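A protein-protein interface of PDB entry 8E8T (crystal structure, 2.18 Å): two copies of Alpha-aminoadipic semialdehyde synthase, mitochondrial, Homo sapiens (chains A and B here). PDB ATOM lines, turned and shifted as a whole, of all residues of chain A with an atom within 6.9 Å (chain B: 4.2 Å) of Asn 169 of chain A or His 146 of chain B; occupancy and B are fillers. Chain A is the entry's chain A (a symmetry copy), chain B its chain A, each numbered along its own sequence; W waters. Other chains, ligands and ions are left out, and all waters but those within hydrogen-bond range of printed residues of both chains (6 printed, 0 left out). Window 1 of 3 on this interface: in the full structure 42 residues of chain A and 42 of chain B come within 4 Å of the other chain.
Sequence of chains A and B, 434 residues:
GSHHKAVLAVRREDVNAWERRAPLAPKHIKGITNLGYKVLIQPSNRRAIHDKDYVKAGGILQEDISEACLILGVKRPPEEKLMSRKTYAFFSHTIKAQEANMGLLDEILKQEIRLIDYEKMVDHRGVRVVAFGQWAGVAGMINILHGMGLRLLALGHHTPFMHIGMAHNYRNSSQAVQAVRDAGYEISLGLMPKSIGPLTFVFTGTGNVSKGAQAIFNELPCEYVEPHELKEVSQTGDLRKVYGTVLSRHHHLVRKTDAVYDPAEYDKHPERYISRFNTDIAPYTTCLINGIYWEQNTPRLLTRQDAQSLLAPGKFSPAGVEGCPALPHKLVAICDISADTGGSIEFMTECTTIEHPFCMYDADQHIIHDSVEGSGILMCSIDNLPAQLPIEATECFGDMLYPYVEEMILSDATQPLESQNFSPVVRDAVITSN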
ATOM      1  N   TRP A  18      21.289 -28.363  -8.357  1.00  0.00           N
ATOM      2  CA  TRP A  18      22.146 -28.537  -9.524  1.00  0.00           C
ATOM      3  C   TRP A  18      21.731 -29.698 -10.413  1.00  0.00           C
ATOM      4  O   TRP A  18      22.410 -29.960 -11.411  1.00  0.00           O
ATOM      5  CB  TRP A  18      23.605 -28.728  -9.094  1.00  0.00           C
ATOM      6  CG  TRP A  18      24.232 -27.491  -8.531  1.00  0.00           C
ATOM      7  CD1 TRP A  18      24.324 -27.154  -7.214  1.00  0.00           C
ATOM      8  CD2 TRP A  18      24.845 -26.419  -9.264  1.00  0.00           C
ATOM      9  NE1 TRP A  18      24.961 -25.944  -7.077  1.00  0.00           N
ATOM     10  CE2 TRP A  18      25.291 -25.471  -8.320  1.00  0.00           C
ATOM     11  CE3 TRP A  18      25.065 -26.171 -10.622  1.00  0.00           C
ATOM     12  CZ2 TRP A  18      25.941 -24.294  -8.690  1.00  0.00           C
ATOM     13  CZ3 TRP A  18      25.711 -24.996 -10.988  1.00  0.00           C
ATOM     14  CH2 TRP A  18      26.139 -24.075 -10.025  1.00  0.00           C
ATOM     15  N   ARG A  20      19.940 -30.488 -13.108  1.00  0.00           N
ATOM     16  CA  ARG A  20      19.289 -29.881 -14.258  1.00  0.00           C
ATOM     17  C   ARG A  20      19.135 -30.849 -15.421  1.00  0.00           C
ATOM     18  O   ARG A  20      18.622 -30.459 -16.473  1.00  0.00           O
ATOM     19  CB  ARG A  20      20.077 -28.643 -14.710  1.00  0.00           C
ATOM     20  CG  ARG A  20      20.242 -27.579 -13.625  1.00  0.00           C
ATOM     21  CD  ARG A  20      21.012 -26.357 -14.131  1.00  0.00           C
ATOM     22  NE  ARG A  20      22.431 -26.645 -14.302  1.00  0.00           N
ATOM     23  CZ  ARG A  20      23.252 -25.952 -15.085  1.00  0.00           C
ATOM     24  NH1 ARG A  20      22.799 -24.920 -15.785  1.00  0.00           N
ATOM     25  NH2 ARG A  20      24.526 -26.299 -15.177  1.00  0.00           N
ATOM     26  N   HIS A 146      40.385 -24.562 -15.262  1.00  0.00           N
ATOM     27  CA  HIS A 146      39.976 -23.394 -14.493  1.00  0.00           C
ATOM     28  C   HIS A 146      40.639 -23.390 -13.121  1.00  0.00           C
ATOM     29  O   HIS A 146      41.173 -22.364 -12.682  1.00  0.00           O
ATOM     30  CB  HIS A 146      38.450 -23.381 -14.369  1.00  0.00           C
ATOM     31  CG  HIS A 146      37.927 -22.444 -13.327  1.00  0.00           C
ATOM     32  ND1 HIS A 146      37.808 -21.086 -13.537  1.00  0.00           N
ATOM     33  CD2 HIS A 146      37.488 -22.671 -12.066  1.00  0.00           C
ATOM     34  CE1 HIS A 146      37.318 -20.516 -12.449  1.00  0.00           C
ATOM     35  NE2 HIS A 146      37.119 -21.456 -11.541  1.00  0.00           N
ATOM     36  N   ILE A 164      39.642 -19.490 -18.496  1.00  0.00           N
ATOM     37  CA  ILE A 164      38.743 -20.628 -18.638  1.00  0.00           C
ATOM     38  C   ILE A 164      37.896 -20.685 -17.373  1.00  0.00           C
ATOM     39  O   ILE A 164      38.439 -20.789 -16.266  1.00  0.00           O
ATOM     40  CB  ILE A 164      39.509 -21.944 -18.852  1.00  0.00           C
ATOM     41  CG1 ILE A 164      40.449 -21.836 -20.053  1.00  0.00           C
ATOM     42  CG2 ILE A 164      38.530 -23.104 -19.055  1.00  0.00           C
ATOM     43  CD1 ILE A 164      41.416 -22.985 -20.182  1.00  0.00           C
ATOM     44  N   GLY A 165      36.576 -20.600 -17.531  1.00  0.00           N
ATOM     45  CA  GLY A 165      35.660 -20.682 -16.412  1.00  0.00           C
ATOM     46  C   GLY A 165      35.377 -22.118 -16.010  1.00  0.00           C
ATOM     47  O   GLY A 165      35.978 -23.067 -16.514  1.00  0.00           O
ATOM     48  N   MET A 166      34.442 -22.272 -15.070  1.00  0.00           N
ATOM     49  CA  MET A 166      33.960 -23.601 -14.716  1.00  0.00           C
ATOM     50  C   MET A 166      33.091 -24.156 -15.842  1.00  0.00           C
ATOM     51  O   MET A 166      32.505 -23.410 -16.632  1.00  0.00           O
ATOM     52  CB  MET A 166      33.157 -23.564 -13.411  1.00  0.00           C
ATOM     53  CG  MET A 166      33.971 -23.255 -12.152  1.00  0.00           C
ATOM     54  SD  MET A 166      34.850 -24.693 -11.499  1.00  0.00           S
ATOM     55  CE  MET A 166      33.505 -25.857 -11.308  1.00  0.00           C
ATOM     56  N   ALA A 167      33.005 -25.486 -15.907  1.00  0.00           N
ATOM     57  CA  ALA A 167      32.231 -26.121 -16.970  1.00  0.00           C
ATOM     58  C   ALA A 167      30.812 -25.565 -17.037  1.00  0.00           C
ATOM     59  O   ALA A 167      30.314 -25.251 -18.126  1.00  0.00           O
ATOM     60  CB  ALA A 167      32.204 -27.637 -16.772  1.00  0.00           C
ATOM     61  N   HIS A 168      30.158 -25.395 -15.882  1.00  0.00           N
ATOM     62  CA  HIS A 168      28.767 -24.944 -15.864  1.00  0.00           C
ATOM     63  C   HIS A 168      28.613 -23.461 -16.192  1.00  0.00           C
ATOM     64  O   HIS A 168      27.475 -22.986 -16.291  1.00  0.00           O
ATOM     65  CB  HIS A 168      28.124 -25.258 -14.502  1.00  0.00           C
ATOM     66  CG  HIS A 168      28.801 -24.602 -13.338  1.00  0.00           C
ATOM     67  ND1 HIS A 168      29.755 -25.242 -12.576  1.00  0.00           N
ATOM     68  CD2 HIS A 168      28.644 -23.376 -12.788  1.00  0.00           C
ATOM     69  CE1 HIS A 168      30.168 -24.435 -11.617  1.00  0.00           C
ATOM     70  NE2 HIS A 168      29.507 -23.296 -11.722  1.00  0.00           N
ATOM     71  N   ASN A 169      29.719 -22.724 -16.365  1.00  0.00           N
ATOM     72  CA  ASN A 169      29.664 -21.335 -16.818  1.00  0.00           C
ATOM     73  C   ASN A 169      29.534 -21.222 -18.331  1.00  0.00           C
ATOM     74  O   ASN A 169      29.465 -20.101 -18.847  1.00  0.00           O
ATOM     75  CB  ASN A 169      30.913 -20.551 -16.404  1.00  0.00           C
ATOM     76  CG  ASN A 169      31.009 -20.319 -14.910  1.00  0.00           C
ATOM     77  OD1 ASN A 169      32.109 -20.289 -14.354  1.00  0.00           O
ATOM     78  ND2 ASN A 169      29.864 -20.141 -14.254  1.00  0.00           N
ATOM     79  N   TYR A 170      29.538 -22.344 -19.045  1.00  0.00           N
ATOM     80  CA  TYR A 170      29.433 -22.378 -20.494  1.00  0.00           C
ATOM     81  C   TYR A 170      28.102 -22.999 -20.902  1.00  0.00           C
ATOM     82  O   TYR A 170      27.621 -23.943 -20.268  1.00  0.00           O
ATOM     83  CB  TYR A 170      30.606 -23.161 -21.091  1.00  0.00           C
ATOM     84  CG  TYR A 170      31.957 -22.532 -20.809  1.00  0.00           C
ATOM     85  CD1 TYR A 170      32.383 -21.417 -21.518  1.00  0.00           C
ATOM     86  CD2 TYR A 170      32.803 -23.047 -19.829  1.00  0.00           C
ATOM     87  CE1 TYR A 170      33.612 -20.835 -21.269  1.00  0.00           C
ATOM     88  CE2 TYR A 170      34.037 -22.463 -19.573  1.00  0.00           C
ATOM     89  CZ  TYR A 170      34.434 -21.360 -20.298  1.00  0.00           C
ATOM     90  OH  TYR A 170      35.648 -20.771 -20.052  1.00  0.00           O
ATOM     91  N   ARG A 171      27.501 -22.440 -21.962  1.00  0.00           N
ATOM     92  CA  ARG A 171      26.219 -22.950 -22.445  1.00  0.00           C
ATOM     93  C   ARG A 171      26.320 -24.421 -22.834  1.00  0.00           C
ATOM     94  O   ARG A 171      25.434 -25.220 -22.510  1.00  0.00           O
ATOM     95  CB  ARG A 171      25.725 -22.119 -23.634  1.00  0.00           C
ATOM     96  CG  ARG A 171      24.350 -22.539 -24.195  1.00  0.00           C
ATOM     97  CD  ARG A 171      23.923 -21.691 -25.401  1.00  0.00           C
ATOM     98  NE  ARG A 171      24.754 -21.952 -26.574  1.00  0.00           N
ATOM     99  CZ  ARG A 171      25.804 -21.218 -26.936  1.00  0.00           C
ATOM    100  NH1 ARG A 171      26.160 -20.151 -26.224  1.00  0.00           N
ATOM    101  NH2 ARG A 171      26.499 -21.548 -28.017  1.00  0.00           N
ATOM    102  N   ASN A 172      27.393 -24.797 -23.528  1.00  0.00           N
ATOM    103  CA  ASN A 172      27.606 -26.173 -23.958  1.00  0.00           C
ATOM    104  C   ASN A 172      29.100 -26.383 -24.189  1.00  0.00           C
ATOM    105  O   ASN A 172      29.915 -25.479 -23.982  1.00  0.00           O
ATOM    106  CB  ASN A 172      26.782 -26.493 -25.211  1.00  0.00           C
ATOM    107  CG  ASN A 172      27.025 -25.517 -26.348  1.00  0.00           C
ATOM    108  OD1 ASN A 172      28.076 -24.881 -26.427  1.00  0.00           O
ATOM    109  ND2 ASN A 172      26.046 -25.394 -27.241  1.00  0.00           N
ATOM    110  N   GLN A 175      30.861 -23.849 -26.742  1.00  0.00           N
ATOM    111  CA  GLN A 175      31.277 -22.558 -26.203  1.00  0.00           C
ATOM    112  C   GLN A 175      32.476 -22.717 -25.276  1.00  0.00           C
ATOM    113  O   GLN A 175      33.368 -21.859 -25.248  1.00  0.00           O
ATOM    114  CB  GLN A 175      30.112 -21.890 -25.469  1.00  0.00           C
ATOM    115  CG  GLN A 175      30.346 -20.417 -25.144  1.00  0.00           C
ATOM    116  CD  GLN A 175      29.315 -19.853 -24.185  1.00  0.00           C
ATOM    117  OE1 GLN A 175      28.917 -20.513 -23.225  1.00  0.00           O
ATOM    118  NE2 GLN A 175      28.876 -18.626 -24.443  1.00  0.00           N
ATOM    119  N   GLN A 388      27.042 -30.533 -15.013  1.00  0.00           N
ATOM    120  CA  GLN A 388      27.563 -29.217 -15.379  1.00  0.00           C
ATOM    121  C   GLN A 388      27.376 -28.919 -16.860  1.00  0.00           C
ATOM    122  O   GLN A 388      27.442 -27.753 -17.259  1.00  0.00           O
ATOM    123  CB  GLN A 388      29.048 -29.113 -15.037  1.00  0.00           C
ATOM    124  CG  GLN A 388      29.358 -29.260 -13.564  1.00  0.00           C
ATOM    125  CD  GLN A 388      30.819 -29.007 -13.269  1.00  0.00           C
ATOM    126  OE1 GLN A 388      31.655 -29.900 -13.401  1.00  0.00           O
ATOM    127  NE2 GLN A 388      31.141 -27.775 -12.888  1.00  0.00           N
ATOM    128  N   ILE B 142      29.250  -7.730 -15.492  1.00  0.00           N
ATOM    129  CA  ILE B 142      29.478  -9.151 -15.744  1.00  0.00           C
ATOM    130  C   ILE B 142      29.319  -9.954 -14.455  1.00  0.00           C
ATOM    131  O   ILE B 142      28.603 -10.964 -14.426  1.00  0.00           O
ATOM    132  CB  ILE B 142      30.865  -9.371 -16.378  1.00  0.00           C
ATOM    133  CG1 ILE B 142      30.988  -8.609 -17.702  1.00  0.00           C
ATOM    134  CG2 ILE B 142      31.128 -10.864 -16.591  1.00  0.00           C
ATOM    135  CD1 ILE B 142      32.431  -8.275 -18.088  1.00  0.00           C
ATOM    136  N   ASN B 143      29.974  -9.516 -13.370  1.00  0.00           N
ATOM    137  CA  ASN B 143      29.868 -10.232 -12.100  1.00  0.00           C
ATOM    138  C   ASN B 143      28.414 -10.378 -11.664  1.00  0.00           C
ATOM    139  O   ASN B 143      27.986 -11.466 -11.264  1.00  0.00           O
ATOM    140  CB  ASN B 143      30.661  -9.521 -10.996  1.00  0.00           C
ATOM    141  CG  ASN B 143      32.166  -9.505 -11.244  1.00  0.00           C
ATOM    142  OD1 ASN B 143      32.716 -10.349 -11.957  1.00  0.00           O
ATOM    143  ND2 ASN B 143      32.839  -8.537 -10.638  1.00  0.00           N
ATOM    144  N   ILE B 144      27.637  -9.294 -11.727  1.00  0.00           N
ATOM    145  CA  ILE B 144      26.277  -9.361 -11.197  1.00  0.00           C
ATOM    146  C   ILE B 144      25.392 -10.242 -12.078  1.00  0.00           C
ATOM    147  O   ILE B 144      24.490 -10.922 -11.573  1.00  0.00           O
ATOM    148  CB  ILE B 144      25.693  -7.945 -10.999  1.00  0.00           C
ATOM    149  CG1 ILE B 144      24.488  -7.991 -10.052  1.00  0.00           C
ATOM    150  CG2 ILE B 144      25.302  -7.300 -12.321  1.00  0.00           C
ATOM    151  CD1 ILE B 144      24.827  -8.489  -8.668  1.00  0.00           C
ATOM    152  N   LEU B 145      25.635 -10.268 -13.391  1.00  0.00           N
ATOM    153  CA  LEU B 145      24.899 -11.194 -14.251  1.00  0.00           C
ATOM    154  C   LEU B 145      25.255 -12.642 -13.925  1.00  0.00           C
ATOM    155  O   LEU B 145      24.379 -13.513 -13.887  1.00  0.00           O
ATOM    156  CB  LEU B 145      25.183 -10.889 -15.720  1.00  0.00           C
ATOM    157  CG  LEU B 145      24.670  -9.529 -16.213  1.00  0.00           C
ATOM    158  CD1 LEU B 145      25.143  -9.235 -17.629  1.00  0.00           C
ATOM    159  CD2 LEU B 145      23.145  -9.479 -16.135  1.00  0.00           C
ATOM    160  N   HIS B 146      26.544 -12.913 -13.705  1.00  0.00           N
ATOM    161  CA  HIS B 146      26.969 -14.227 -13.241  1.00  0.00           C
ATOM    162  C   HIS B 146      26.340 -14.555 -11.892  1.00  0.00           C
ATOM    163  O   HIS B 146      25.814 -15.656 -11.693  1.00  0.00           O
ATOM    164  CB  HIS B 146      28.498 -14.265 -13.162  1.00  0.00           C
ATOM    165  CG  HIS B 146      29.043 -15.418 -12.381  1.00  0.00           C
ATOM    166  ND1 HIS B 146      29.153 -16.689 -12.906  1.00  0.00           N
ATOM    167  CD2 HIS B 146      29.514 -15.492 -11.114  1.00  0.00           C
ATOM    168  CE1 HIS B 146      29.668 -17.496 -11.994  1.00  0.00           C
ATOM    169  NE2 HIS B 146      29.892 -16.795 -10.897  1.00  0.00           N
ATOM    170  N   GLY B 147      26.359 -13.598 -10.963  1.00  0.00           N
ATOM    171  CA  GLY B 147      25.760 -13.831  -9.659  1.00  0.00           C
ATOM    172  C   GLY B 147      24.262 -14.056  -9.722  1.00  0.00           C
ATOM    173  O   GLY B 147      23.708 -14.816  -8.925  1.00  0.00           O
ATOM    174  N   MET B 148      23.583 -13.394 -10.659  1.00  0.00           N
ATOM    175  CA  MET B 148      22.142 -13.591 -10.770  1.00  0.00           C
ATOM    176  C   MET B 148      21.819 -14.995 -11.261  1.00  0.00           C
ATOM    177  O   MET B 148      20.827 -15.597 -10.831  1.00  0.00           O
ATOM    178  CB  MET B 148      21.531 -12.533 -11.685  1.00  0.00           C
ATOM    179  CG  MET B 148      21.310 -11.211 -10.978  1.00  0.00           C
ATOM    180  SD  MET B 148      20.564  -9.995 -12.062  1.00  0.00           S
ATOM    181  CE  MET B 148      19.018 -10.810 -12.452  1.00  0.00           C
ATOM    182  N   GLY B 149      22.660 -15.546 -12.142  1.00  0.00           N
ATOM    183  CA  GLY B 149      22.473 -16.926 -12.567  1.00  0.00           C
ATOM    184  C   GLY B 149      22.577 -17.909 -11.416  1.00  0.00           C
ATOM    185  O   GLY B 149      21.736 -18.799 -11.265  1.00  0.00           O
ATOM    186  N   LEU B 150      23.616 -17.761 -10.588  1.00  0.00           N
ATOM    187  CA  LEU B 150      23.780 -18.647  -9.438  1.00  0.00           C
ATOM    188  C   LEU B 150      22.642 -18.469  -8.440  1.00  0.00           C
ATOM    189  O   LEU B 150      22.086 -19.454  -7.939  1.00  0.00           O
ATOM    190  CB  LEU B 150      25.125 -18.393  -8.758  1.00  0.00           C
ATOM    191  CG  LEU B 150      26.391 -18.817  -9.507  1.00  0.00           C
ATOM    192  CD1 LEU B 150      27.634 -18.540  -8.666  1.00  0.00           C
ATOM    193  CD2 LEU B 150      26.320 -20.283  -9.888  1.00  0.00           C
ATOM    194  N   MET B 162      23.281 -18.466 -16.187  1.00  0.00           N
ATOM    195  CA  MET B 162      24.228 -19.507 -15.805  1.00  0.00           C
ATOM    196  C   MET B 162      25.404 -19.599 -16.768  1.00  0.00           C
ATOM    197  O   MET B 162      26.441 -20.175 -16.418  1.00  0.00           O
ATOM    198  CB  MET B 162      23.506 -20.863 -15.742  1.00  0.00           C
ATOM    199  CG  MET B 162      22.607 -21.034 -14.526  1.00  0.00           C
ATOM    200  SD  MET B 162      23.574 -21.154 -13.010  1.00  0.00           S
ATOM    201  CE  MET B 162      24.627 -22.553 -13.407  1.00  0.00           C
ATOM    202  N   HIS B 163      25.271 -19.043 -17.970  1.00  0.00           N
ATOM    203  CA  HIS B 163      26.289 -19.140 -19.004  1.00  0.00           C
ATOM    204  C   HIS B 163      27.105 -17.859 -19.133  1.00  0.00           C
ATOM    205  O   HIS B 163      27.648 -17.572 -20.206  1.00  0.00           O
ATOM    206  CB  HIS B 163      25.628 -19.522 -20.326  1.00  0.00           C
ATOM    207  CG  HIS B 163      24.729 -20.715 -20.208  1.00  0.00           C
ATOM    208  ND1 HIS B 163      23.595 -20.878 -20.973  1.00  0.00           N
ATOM    209  CD2 HIS B 163      24.793 -21.796 -19.395  1.00  0.00           C
ATOM    210  CE1 HIS B 163      23.006 -22.016 -20.646  1.00  0.00           C
ATOM    211  NE2 HIS B 163      23.712 -22.591 -19.690  1.00  0.00           N
ATOM    212  N   ILE B 164      27.193 -17.084 -18.055  1.00  0.00           N
ATOM    213  CA  ILE B 164      28.091 -15.942 -17.948  1.00  0.00           C
ATOM    214  C   ILE B 164      28.969 -16.180 -16.727  1.00  0.00           C
ATOM    215  O   ILE B 164      28.455 -16.341 -15.612  1.00  0.00           O
ATOM    216  CB  ILE B 164      27.324 -14.614 -17.829  1.00  0.00           C
ATOM    217  CG1 ILE B 164      26.355 -14.441 -18.998  1.00  0.00           C
ATOM    218  CG2 ILE B 164      28.301 -13.436 -17.778  1.00  0.00           C
ATOM    219  CD1 ILE B 164      25.389 -13.297 -18.831  1.00  0.00           C
ATOM    220  N   GLY B 165      30.285 -16.222 -16.932  1.00  0.00           N
ATOM    221  CA  GLY B 165      31.228 -16.402 -15.848  1.00  0.00           C
ATOM    222  C   GLY B 165      31.526 -15.099 -15.128  1.00  0.00           C
ATOM    223  O   GLY B 165      30.916 -14.060 -15.380  1.00  0.00           O
ATOM    224  N   MET B 166      32.484 -15.167 -14.201  1.00  0.00           N
ATOM    225  CA  MET B 166      32.978 -13.956 -13.558  1.00  0.00           C
ATOM    226  C   MET B 166      33.821 -13.151 -14.543  1.00  0.00           C
ATOM    227  O   MET B 166      34.385 -13.689 -15.500  1.00  0.00           O
ATOM    228  CB  MET B 166      33.813 -14.295 -12.318  1.00  0.00           C
ATOM    229  CG  MET B 166      33.029 -14.894 -11.147  1.00  0.00           C
ATOM    230  SD  MET B 166      32.171 -13.651 -10.154  1.00  0.00           S
ATOM    231  CE  MET B 166      33.524 -12.560  -9.729  1.00  0.00           C
ATOM    232  N   ASN B 169      37.175 -14.411 -15.470  1.00  0.00           N
ATOM    233  CA  ASN B 169      37.215 -15.655 -16.238  1.00  0.00           C
ATOM    234  C   ASN B 169      37.307 -15.409 -17.737  1.00  0.00           C
ATOM    235  O   ASN B 169      37.360 -16.378 -18.504  1.00  0.00           O
ATOM    236  CB  ASN B 169      35.974 -16.517 -15.988  1.00  0.00           C
ATOM    237  CG  ASN B 169      35.914 -17.093 -14.589  1.00  0.00           C
ATOM    238  OD1 ASN B 169      34.828 -17.256 -14.027  1.00  0.00           O
ATOM    239  ND2 ASN B 169      37.074 -17.417 -14.020  1.00  0.00           N
ATOM    240  N   PHE B 358      30.212 -12.547  -3.719  1.00  0.00           N
ATOM    241  CA  PHE B 358      28.813 -12.323  -3.381  1.00  0.00           C
ATOM    242  C   PHE B 358      28.550 -12.625  -1.911  1.00  0.00           C
ATOM    243  O   PHE B 358      29.192 -13.490  -1.310  1.00  0.00           O
ATOM    244  CB  PHE B 358      27.893 -13.180  -4.268  1.00  0.00           C
ATOM    245  CG  PHE B 358      28.200 -13.068  -5.740  1.00  0.00           C
ATOM    246  CD1 PHE B 358      27.971 -11.882  -6.421  1.00  0.00           C
ATOM    247  CD2 PHE B 358      28.712 -14.150  -6.440  1.00  0.00           C
ATOM    248  CE1 PHE B 358      28.255 -11.774  -7.771  1.00  0.00           C
ATOM    249  CE2 PHE B 358      28.998 -14.050  -7.793  1.00  0.00           C
ATOM    250  CZ  PHE B 358      28.774 -12.857  -8.456  1.00  0.00           C
HETATM  251  O   HOH W   1      36.087 -18.147 -20.681  1.00  0.00           O
HETATM  252  O   HOH W   2      30.689 -17.868 -20.580  1.00  0.00           O
HETATM  253  O   HOH W   3      22.880 -25.399 -18.943  1.00  0.00           O
HETATM  254  O   HOH W   4      26.924 -17.166 -22.515  1.00  0.00           O
HETATM  255  O   HOH W   5      25.212 -24.442 -17.213  1.00  0.00           O
HETATM  256  O   HOH W   6      27.432 -20.338 -13.946  1.00  0.00           O
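The backbone carbonyl oxygen (O) of His 168 of chain A sits close to the backbone carbonyl oxygen (O) of Met 162 of chain B (3.0 Å).
O of His 163 of chain B sits close to O of Asn 169 of chain A, at 3.4 Å.
O of Ile 164 of chain B sits at hydrogen-bond distance from ND1 of His 146 of chain B.
The side-chain amide oxygen (OD1) of Asn 169 of chain B sits at hydrogen-bond distance from the backbone NH (N) of Met 166 of chain B (3.1 Å).
The backbone NH (N) of Gly 165 of chain A sits at hydrogen-bond distance from the side-chain hydroxyl (OH) of Tyr 170 of chain A, at 2.7 Å.
OD1 of Asn 169 of chain A sits at hydrogen-bond distance from N of Met 166 of chain A, 3.1 Å away.
A ring nitrogen (ND1) of His 168 of chain A lies within hydrogen-bond range of the side-chain amide nitrogen (NE2) of Gln 388 of chain A (2.9 Å).
OE1 of Gln 175 of chain A sits at hydrogen-bond distance from N of Arg 171 of chain A (2.7 Å).
Among the printed residues, pairs that only touch across the chains: Asn 169 of chain A with Met 162 of chain B (3.4 Å), His 146 of chain A with Asn 169 of chain B (3.5 Å), Asn 169 of chain A with His 146 of chain B (3.5 Å), Arg 171 of chain A with His 163 of chain B (3.5 Å), Trp 18 of chain A with Met 162 of chain B (3.6 Å), Tyr 170 of chain A with His 163 of chain B (3.7 Å), Trp 18 of chain A with Leu 150 of chain B (3.8 Å), Arg 20 of chain A with Met 162 of chain B (3.8 Å), Asn 169 of chain A with Ile 164 of chain B (3.9 Å) and Ile 164 of chain A with Asn 169 of chain B (3.9 Å).
Of the printed residues of chain B, Asn 169 of chain A touches His 146 (3.5 Å), Met 162 (3.4 Å), His 163 (3.3 Å) and Ile 164 (3.9 Å).
Of chain A, only Asn 169 comes within 4 Å of His 146 of chain B.
Of the printed residues of chain A, Asn 169 of chain B touches His 146 and Ile 164.
Printed residues of chain A within 4 Å of Met 162 of chain B: Trp 18, Arg 20, His 168 and Asn 169.
The nearest residue of chain B that does not touch Asn 169 of chain A is Gly 165 of chain B (4.03 Å).
The nearest residue of chain A that does not touch His 146 of chain B is His 168 of chain A (5.8 Å).
The nearest printed residue of chain B that does not touch Arg 171 of chain A is Met 162 of chain B (6.1 Å).
Of the 16 printed residues of chain B, 6 touch a printed residue of chain A.
Printed residues of chain B that touch a printed residue of chain A: His 146, Leu 150, Met 162, His 163, Ile 164 and Asn 169.
Along chain B the printed residues that touch a printed residue of chain A span positions 146 to 169.
Printed residues of chain A that touch a printed residue of chain B: Trp 18, Arg 20, His 146, Ile 164, His 168, Asn 169, Tyr 170 and Arg 171.
Hydrophobic or aromatic side chains of chain A within 4 Å of the printed part of chain B: Trp 18 and His 146.
Among the printed residues, no Asp or Glu carboxylate lies within 4 Å of a Lys or Arg side-chain nitrogen of the other chain.
His 146 of chain A touches Asn 169 of chain B, and with the chains exchanged Asn 169 of chain A touches His 146 of chain B.
Ile 164 of chain A touches Asn 169 of chain B, and with the chains exchanged Asn 169 of chain A touches Ile 164 of chain B.
Of the 12 pairs that touch across the chains among the printed residues, 4 have their exchanged pair printed and touching as well.
Water W4 bridges the backbone carbonyl oxygen (O) of His 163 of chain B (2.5 Å) and the side-chain amide nitrogen (NE2) of Gln 175 of chain A (3.1 Å).
Water W6 bridges the side-chain amide nitrogen of Asn 169 of chain A (2.5 Å) and the backbone carbonyl oxygen of Met 162 of chain B (2.7 Å).
Water W1 bridges OH of Tyr 170 of chain A and O of Asn 169 of chain B.
Water W5 lies within hydrogen-bond range of the guanidinium group (NH2) of Arg 20 of chain A, the backbone carbonyl oxygen (O) of His 168 of chain A and a ring nitrogen (NE2) of His 163 of chain B.
Water W3 lies within hydrogen-bond range of NE2 of His 163 of chain B (3.0 Å) and NH1 of Arg 20 of chain A (3.2 Å).
Water W2 bridges the backbone carbonyl oxygen of His 163 of chain B (3.1 Å) and the backbone carbonyl oxygen of Asn 169 of chain A (3.1 Å).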
